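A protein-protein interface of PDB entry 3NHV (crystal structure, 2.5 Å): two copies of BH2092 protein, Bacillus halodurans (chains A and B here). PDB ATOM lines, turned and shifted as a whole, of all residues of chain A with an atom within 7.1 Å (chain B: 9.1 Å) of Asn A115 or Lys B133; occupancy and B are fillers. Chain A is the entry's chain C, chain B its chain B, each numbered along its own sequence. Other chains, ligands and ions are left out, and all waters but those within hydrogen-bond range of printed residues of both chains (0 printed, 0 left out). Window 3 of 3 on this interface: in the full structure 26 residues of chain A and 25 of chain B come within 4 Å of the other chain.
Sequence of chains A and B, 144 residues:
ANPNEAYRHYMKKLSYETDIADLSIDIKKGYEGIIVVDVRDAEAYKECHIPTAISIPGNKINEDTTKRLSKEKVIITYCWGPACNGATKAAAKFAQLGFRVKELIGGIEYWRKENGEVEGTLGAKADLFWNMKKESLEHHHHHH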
ATOM      1  N   SER A  24       2.237  10.093 -16.531  1.00  0.00           N
ATOM      2  CA  SER A  24       1.814  10.784 -17.737  1.00  0.00           C
ATOM      3  C   SER A  24       0.408  11.359 -17.601  1.00  0.00           C
ATOM      4  O   SER A  24       0.103  12.411 -18.165  1.00  0.00           O
ATOM      5  CB  SER A  24       1.869   9.827 -18.920  1.00  0.00           C
ATOM      6  OG  SER A  24       1.061   8.696 -18.669  1.00  0.00           O
ATOM      7  N   LYS A  28      -0.679  15.108 -17.872  1.00  0.00           N
ATOM      8  CA  LYS A  28      -1.613  15.509 -18.923  1.00  0.00           C
ATOM      9  C   LYS A  28      -2.761  16.344 -18.369  1.00  0.00           C
ATOM     10  O   LYS A  28      -3.129  17.366 -18.951  1.00  0.00           O
ATOM     11  CB  LYS A  28      -2.195  14.285 -19.658  1.00  0.00           C
ATOM     12  CG  LYS A  28      -1.397  13.852 -20.900  1.00  0.00           C
ATOM     13  CD  LYS A  28      -2.224  12.977 -21.857  1.00  0.00           C
ATOM     14  CE  LYS A  28      -1.428  12.572 -23.115  1.00  0.00           C
ATOM     15  NZ  LYS A  28      -0.250  11.671 -22.831  1.00  0.00           N
ATOM     16  N   TYR A 110      12.366   4.973 -19.476  1.00  0.00           N
ATOM     17  CA  TYR A 110      11.142   4.421 -20.021  1.00  0.00           C
ATOM     18  C   TYR A 110      10.105   5.483 -20.350  1.00  0.00           C
ATOM     19  O   TYR A 110       9.183   5.236 -21.130  1.00  0.00           O
ATOM     20  CB  TYR A 110      10.584   3.346 -19.087  1.00  0.00           C
ATOM     21  CG  TYR A 110      11.118   1.976 -19.454  1.00  0.00           C
ATOM     22  CD1 TYR A 110      10.403   1.136 -20.310  1.00  0.00           C
ATOM     23  CD2 TYR A 110      12.373   1.553 -19.014  1.00  0.00           C
ATOM     24  CE1 TYR A 110      10.927  -0.088 -20.720  1.00  0.00           C
ATOM     25  CE2 TYR A 110      12.906   0.335 -19.420  1.00  0.00           C
ATOM     26  CZ  TYR A 110      12.181  -0.481 -20.272  1.00  0.00           C
ATOM     27  OH  TYR A 110      12.716  -1.682 -20.680  1.00  0.00           O
ATOM     28  N   TRP A 111      10.272   6.671 -19.769  1.00  0.00           N
ATOM     29  CA  TRP A 111       9.373   7.786 -20.048  1.00  0.00           C
ATOM     30  C   TRP A 111       9.562   8.111 -21.525  1.00  0.00           C
ATOM     31  O   TRP A 111       8.623   8.511 -22.206  1.00  0.00           O
ATOM     32  CB  TRP A 111       9.725   9.012 -19.194  1.00  0.00           C
ATOM     33  CG  TRP A 111       9.024  10.284 -19.636  1.00  0.00           C
ATOM     34  CD1 TRP A 111       9.440  11.167 -20.603  1.00  0.00           C
ATOM     35  CD2 TRP A 111       7.744  10.758 -19.189  1.00  0.00           C
ATOM     36  NE1 TRP A 111       8.494  12.150 -20.786  1.00  0.00           N
ATOM     37  CE2 TRP A 111       7.448  11.923 -19.935  1.00  0.00           C
ATOM     38  CE3 TRP A 111       6.820  10.308 -18.236  1.00  0.00           C
ATOM     39  CZ2 TRP A 111       6.260  12.642 -19.755  1.00  0.00           C
ATOM     40  CZ3 TRP A 111       5.638  11.024 -18.057  1.00  0.00           C
ATOM     41  CH2 TRP A 111       5.370  12.179 -18.816  1.00  0.00           C
ATOM     42  N   ARG A 112      10.780   7.930 -22.022  1.00  0.00           N
ATOM     43  CA  ARG A 112      11.032   8.194 -23.424  1.00  0.00           C
ATOM     44  C   ARG A 112      10.660   6.991 -24.273  1.00  0.00           C
ATOM     45  O   ARG A 112      10.003   7.140 -25.296  1.00  0.00           O
ATOM     46  CB  ARG A 112      12.493   8.559 -23.655  1.00  0.00           C
ATOM     47  CG  ARG A 112      12.897   9.855 -22.998  1.00  0.00           C
ATOM     48  CD  ARG A 112      13.976  10.517 -23.815  1.00  0.00           C
ATOM     49  NE  ARG A 112      15.291  10.432 -23.201  1.00  0.00           N
ATOM     50  CZ  ARG A 112      16.427  10.618 -23.864  1.00  0.00           C
ATOM     51  NH1 ARG A 112      16.398  10.888 -25.163  1.00  0.00           N
ATOM     52  NH2 ARG A 112      17.589  10.549 -23.224  1.00  0.00           N
ATOM     53  N   LYS A 113      11.072   5.797 -23.858  1.00  0.00           N
ATOM     54  CA  LYS A 113      10.745   4.591 -24.614  1.00  0.00           C
ATOM     55  C   LYS A 113       9.235   4.488 -24.764  1.00  0.00           C
ATOM     56  O   LYS A 113       8.732   3.744 -25.602  1.00  0.00           O
ATOM     57  CB  LYS A 113      11.253   3.335 -23.900  1.00  0.00           C
ATOM     58  CG  LYS A 113      12.744   3.065 -24.029  1.00  0.00           C
ATOM     59  CD  LYS A 113      13.130   1.803 -23.252  1.00  0.00           C
ATOM     60  CE  LYS A 113      14.604   1.454 -23.441  1.00  0.00           C
ATOM     61  NZ  LYS A 113      15.035   0.258 -22.647  1.00  0.00           N
ATOM     62  N   GLU A 114       8.515   5.235 -23.939  1.00  0.00           N
ATOM     63  CA  GLU A 114       7.068   5.220 -24.001  1.00  0.00           C
ATOM     64  C   GLU A 114       6.518   6.484 -24.658  1.00  0.00           C
ATOM     65  O   GLU A 114       5.488   7.022 -24.254  1.00  0.00           O
ATOM     66  CB  GLU A 114       6.495   5.009 -22.595  1.00  0.00           C
ATOM     67  CG  GLU A 114       6.544   3.541 -22.195  1.00  0.00           C
ATOM     68  CD  GLU A 114       6.147   3.275 -20.762  1.00  0.00           C
ATOM     69  OE1 GLU A 114       5.115   3.808 -20.309  1.00  0.00           O
ATOM     70  OE2 GLU A 114       6.865   2.511 -20.089  1.00  0.00           O
ATOM     71  N   ASN A 115       7.229   6.938 -25.688  1.00  0.00           N
ATOM     72  CA  ASN A 115       6.860   8.119 -26.463  1.00  0.00           C
ATOM     73  C   ASN A 115       6.478   9.324 -25.601  1.00  0.00           C
ATOM     74  O   ASN A 115       5.499  10.014 -25.883  1.00  0.00           O
ATOM     75  CB  ASN A 115       5.710   7.764 -27.420  1.00  0.00           C
ATOM     76  CG  ASN A 115       5.861   8.411 -28.790  1.00  0.00           C
ATOM     77  OD1 ASN A 115       6.914   8.309 -29.426  1.00  0.00           O
ATOM     78  ND2 ASN A 115       4.805   9.073 -29.255  1.00  0.00           N
ATOM     79  N   GLY A 116       7.252   9.577 -24.552  1.00  0.00           N
ATOM     80  CA  GLY A 116       6.980  10.714 -23.691  1.00  0.00           C
ATOM     81  C   GLY A 116       7.816  11.892 -24.153  1.00  0.00           C
ATOM     82  O   GLY A 116       8.940  11.707 -24.627  1.00  0.00           O
ATOM     83  N   GLU A 117       7.283  13.105 -24.030  1.00  0.00           N
ATOM     84  CA  GLU A 117       8.024  14.292 -24.456  1.00  0.00           C
ATOM     85  C   GLU A 117       8.943  14.786 -23.349  1.00  0.00           C
ATOM     86  O   GLU A 117       8.639  14.642 -22.162  1.00  0.00           O
ATOM     87  CB  GLU A 117       7.066  15.418 -24.870  1.00  0.00           C
ATOM     88  CG  GLU A 117       6.028  15.023 -25.922  1.00  0.00           C
ATOM     89  CD  GLU A 117       6.621  14.232 -27.089  1.00  0.00           C
ATOM     90  OE1 GLU A 117       6.951  13.034 -26.900  1.00  0.00           O
ATOM     91  OE2 GLU A 117       6.763  14.807 -28.194  1.00  0.00           O
ATOM     92  N   PHE B 129       6.845  -1.344 -27.074  1.00  0.00           N
ATOM     93  CA  PHE B 129       6.560  -0.527 -25.903  1.00  0.00           C
ATOM     94  C   PHE B 129       5.165   0.095 -25.934  1.00  0.00           C
ATOM     95  O   PHE B 129       4.544   0.214 -26.985  1.00  0.00           O
ATOM     96  CB  PHE B 129       7.577   0.606 -25.782  1.00  0.00           C
ATOM     97  CG  PHE B 129       9.003   0.158 -25.786  1.00  0.00           C
ATOM     98  CD1 PHE B 129       9.735   0.142 -26.968  1.00  0.00           C
ATOM     99  CD2 PHE B 129       9.629  -0.214 -24.601  1.00  0.00           C
ATOM    100  CE1 PHE B 129      11.083  -0.237 -26.972  1.00  0.00           C
ATOM    101  CE2 PHE B 129      10.970  -0.594 -24.589  1.00  0.00           C
ATOM    102  CZ  PHE B 129      11.703  -0.605 -25.778  1.00  0.00           C
ATOM    103  N   TRP B 130       4.694   0.499 -24.760  1.00  0.00           N
ATOM    104  CA  TRP B 130       3.403   1.150 -24.616  1.00  0.00           C
ATOM    105  C   TRP B 130       3.534   2.559 -25.198  1.00  0.00           C
ATOM    106  O   TRP B 130       4.516   3.254 -24.921  1.00  0.00           O
ATOM    107  CB  TRP B 130       3.042   1.244 -23.138  1.00  0.00           C
ATOM    108  CG  TRP B 130       1.751   1.951 -22.868  1.00  0.00           C
ATOM    109  CD1 TRP B 130       0.499   1.529 -23.213  1.00  0.00           C
ATOM    110  CD2 TRP B 130       1.574   3.183 -22.152  1.00  0.00           C
ATOM    111  NE1 TRP B 130      -0.447   2.414 -22.753  1.00  0.00           N
ATOM    112  CE2 TRP B 130       0.186   3.439 -22.097  1.00  0.00           C
ATOM    113  CE3 TRP B 130       2.454   4.093 -21.549  1.00  0.00           C
ATOM    114  CZ2 TRP B 130      -0.346   4.568 -21.463  1.00  0.00           C
ATOM    115  CZ3 TRP B 130       1.924   5.216 -20.917  1.00  0.00           C
ATOM    116  CH2 TRP B 130       0.536   5.442 -20.881  1.00  0.00           C
ATOM    117  N   ASN B 131       2.551   2.974 -26.001  1.00  0.00           N
ATOM    118  CA  ASN B 131       2.557   4.302 -26.633  1.00  0.00           C
ATOM    119  C   ASN B 131       1.698   5.289 -25.845  1.00  0.00           C
ATOM    120  O   ASN B 131       0.471   5.197 -25.839  1.00  0.00           O
ATOM    121  CB  ASN B 131       2.029   4.214 -28.068  1.00  0.00           C
ATOM    122  CG  ASN B 131       2.470   5.387 -28.932  1.00  0.00           C
ATOM    123  OD1 ASN B 131       2.435   6.547 -28.507  1.00  0.00           O
ATOM    124  ND2 ASN B 131       2.875   5.087 -30.161  1.00  0.00           N
ATOM    125  N   MET B 132       2.354   6.241 -25.196  1.00  0.00           N
ATOM    126  CA  MET B 132       1.676   7.246 -24.385  1.00  0.00           C
ATOM    127  C   MET B 132       0.687   8.099 -25.179  1.00  0.00           C
ATOM    128  O   MET B 132      -0.244   8.673 -24.611  1.00  0.00           O
ATOM    129  CB  MET B 132       2.720   8.149 -23.743  1.00  0.00           C
ATOM    130  CG  MET B 132       2.203   9.064 -22.675  1.00  0.00           C
ATOM    131  SD  MET B 132       3.638  10.212 -22.080  1.00  0.00           S
ATOM    132  CE  MET B 132       4.735   8.900 -21.176  1.00  0.00           C
ATOM    133  N   LYS B 133       0.893   8.187 -26.488  1.00  0.00           N
ATOM    134  CA  LYS B 133       0.009   8.985 -27.326  1.00  0.00           C
ATOM    135  C   LYS B 133      -1.187   8.181 -27.830  1.00  0.00           C
ATOM    136  O   LYS B 133      -2.296   8.704 -27.923  1.00  0.00           O
ATOM    137  CB  LYS B 133       0.776   9.567 -28.521  1.00  0.00           C
ATOM    138  CG  LYS B 133       2.117  10.219 -28.168  1.00  0.00           C
ATOM    139  CD  LYS B 133       2.114  10.910 -26.796  1.00  0.00           C
ATOM    140  CE  LYS B 133       1.145  12.075 -26.714  1.00  0.00           C
ATOM    141  NZ  LYS B 133       1.109  12.634 -25.324  1.00  0.00           N
ATOM    142  N   LYS B 134      -0.966   6.912 -28.156  1.00  0.00           N
ATOM    143  CA  LYS B 134      -2.048   6.064 -28.650  1.00  0.00           C
ATOM    144  C   LYS B 134      -3.268   6.056 -27.728  1.00  0.00           C
ATOM    145  O   LYS B 134      -4.376   5.709 -28.154  1.00  0.00           O
ATOM    146  CB  LYS B 134      -1.568   4.620 -28.845  1.00  0.00           C
ATOM    147  CG  LYS B 134      -1.434   4.181 -30.307  1.00  0.00           C
ATOM    148  CD  LYS B 134      -1.673   2.672 -30.460  1.00  0.00           C
ATOM    149  CE  LYS B 134      -3.108   2.304 -30.046  1.00  0.00           C
ATOM    150  NZ  LYS B 134      -3.434   0.849 -30.098  1.00  0.00           N
ATOM    151  N   GLU B 135      -3.074   6.439 -26.470  1.00  0.00           N
ATOM    152  CA  GLU B 135      -4.175   6.457 -25.517  1.00  0.00           C
ATOM    153  C   GLU B 135      -5.288   7.396 -25.944  1.00  0.00           C
ATOM    154  O   GLU B 135      -6.448   6.981 -26.054  1.00  0.00           O
ATOM    155  CB  GLU B 135      -3.669   6.837 -24.124  1.00  0.00           C
ATOM    156  CG  GLU B 135      -2.907   5.702 -23.457  1.00  0.00           C
ATOM    157  CD  GLU B 135      -3.749   4.434 -23.366  1.00  0.00           C
ATOM    158  OE1 GLU B 135      -4.754   4.444 -22.613  1.00  0.00           O
ATOM    159  OE2 GLU B 135      -3.416   3.438 -24.059  1.00  0.00           O
ATOM    160  N   SER B 136      -4.948   8.660 -26.174  1.00  0.00           N
ATOM    161  CA  SER B 136      -5.957   9.619 -26.618  1.00  0.00           C
ATOM    162  C   SER B 136      -6.622   9.090 -27.899  1.00  0.00           C
ATOM    163  O   SER B 136      -7.805   9.360 -28.148  1.00  0.00           O
ATOM    164  CB  SER B 136      -5.321  10.990 -26.888  1.00  0.00           C
ATOM    165  OG  SER B 136      -4.837  11.588 -25.694  1.00  0.00           O
ATOM    166  N   LEU B 137      -5.868   8.330 -28.701  1.00  0.00           N
ATOM    167  CA  LEU B 137      -6.394   7.767 -29.948  1.00  0.00           C
ATOM    168  C   LEU B 137      -7.034   6.376 -29.760  1.00  0.00           C
ATOM    169  O   LEU B 137      -7.251   5.633 -30.731  1.00  0.00           O
ATOM    170  CB  LEU B 137      -5.292   7.728 -31.026  1.00  0.00           C
ATOM    171  CG  LEU B 137      -4.776   9.111 -31.468  1.00  0.00           C
ATOM    172  CD1 LEU B 137      -3.754   9.616 -30.457  1.00  0.00           C
ATOM    173  CD2 LEU B 137      -4.144   9.030 -32.854  1.00  0.00           C
ATOM    174  N   GLU B 138      -7.335   6.039 -28.502  1.00  0.00           N
ATOM    175  CA  GLU B 138      -7.985   4.772 -28.141  1.00  0.00           C
ATOM    176  C   GLU B 138      -8.463   4.836 -26.683  1.00  0.00           C
ATOM    177  O   GLU B 138      -8.847   5.942 -26.231  1.00  0.00           O
ATOM    178  CB  GLU B 138      -7.039   3.572 -28.330  1.00  0.00           C
ATOM    179  CG  GLU B 138      -7.770   2.302 -28.812  1.00  0.00           C
ATOM    180  CD  GLU B 138      -7.190   0.998 -28.241  1.00  0.00           C
ATOM    181  OE1 GLU B 138      -7.794  -0.081 -28.479  1.00  0.00           O
ATOM    182  OE2 GLU B 138      -6.135   1.050 -27.558  1.00  0.00           O
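NZ of Lys A28 lies within hydrogen-bond range of O of Met B132, 3.5 Å away.
The backbone carbonyl oxygen (O) of Glu A114 sits close to the backbone NH (N) of Met B132.
The side-chain amino group (NZ) of Lys A28 lies close to the side-chain amino group (NZ) of Lys B133 (3.0 Å).
NE1 of Trp B130 is in hydrogen-bond range of OE2 of Glu B135 (3.4 Å).
The indole nitrogen of Trp A111 lies within hydrogen-bond range of the backbone carbonyl oxygen of Glu A117 (2.9 Å).
OD1 of Asn B131 sits at hydrogen-bond distance from N of Lys B134 (3.4 Å).
OD1 of Asn B131 sits at hydrogen-bond distance from N of Lys B133 (3.0 Å).
The backbone NH (N) of Gly A116 lies within hydrogen-bond range of the backbone carbonyl oxygen (O) of Trp A111.
Among the printed residues, merely in contact across the chains: Ser A24 with Trp B130 (3.97 Å), Ser A24 with Met B132 (3.6 Å), Tyr A110 with Phe B129 (3.9 Å), Trp A111 with Met B132 (3.9 Å), Lys A113 with Phe B129 (3.3 Å), Glu A114 with Trp B130 (2.9 Å), Asn A115 with Asn B131 (3.5 Å), Asn A115 with Met B132 (3.97 Å), Asn A115 with Lys B133 (3.1 Å) and Gly A116 with Met B132 (3.7 Å).
Of the printed residues of chain B, Ser A24 touches Trp B130 and Met B132.
Printed residues of chain B within 4 Å of Lys A28: Met B132 (3.5 Å) and Lys B133 (3.0 Å).
Of the printed residues of chain B, Asn A115 touches Asn B131, Met B132 and Lys B133.
Printed residues of chain A within 4 Å of Trp B130: Ser A24 and Glu A114.
Of chain A, only Lys A28 (3.0 Å) and Asn A115 (3.1 Å) come within 4 Å of Lys B133.
Glu B138 touches none of the printed residues of chain A.
The nearest printed residue of chain B that does not touch Tyr A110 is Met B132 (5.8 Å).
Printed residues of chain A that touch a printed residue of chain B: Ser A24, Lys A28, Tyr A110, Trp A111, Lys A113, Glu A114, Asn A115 and Gly A116.
Hydrophobic or aromatic side chains of chain A that line the printed part of chain B: Tyr A110 and Trp A111.
Printed residues of chain B that touch a printed residue of chain A: Phe B129, Trp B130, Asn B131, Met B132 and Lys B133.
Hydrophobic or aromatic side chains of chain B within 4 Å of the printed part of chain A: Phe B129, Trp B130 and Met B132.
Among the printed residues, no Asp or Glu carboxylate lies within 4 Å of a Lys or Arg side-chain nitrogen of the other chain.
No position is printed for both chains.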
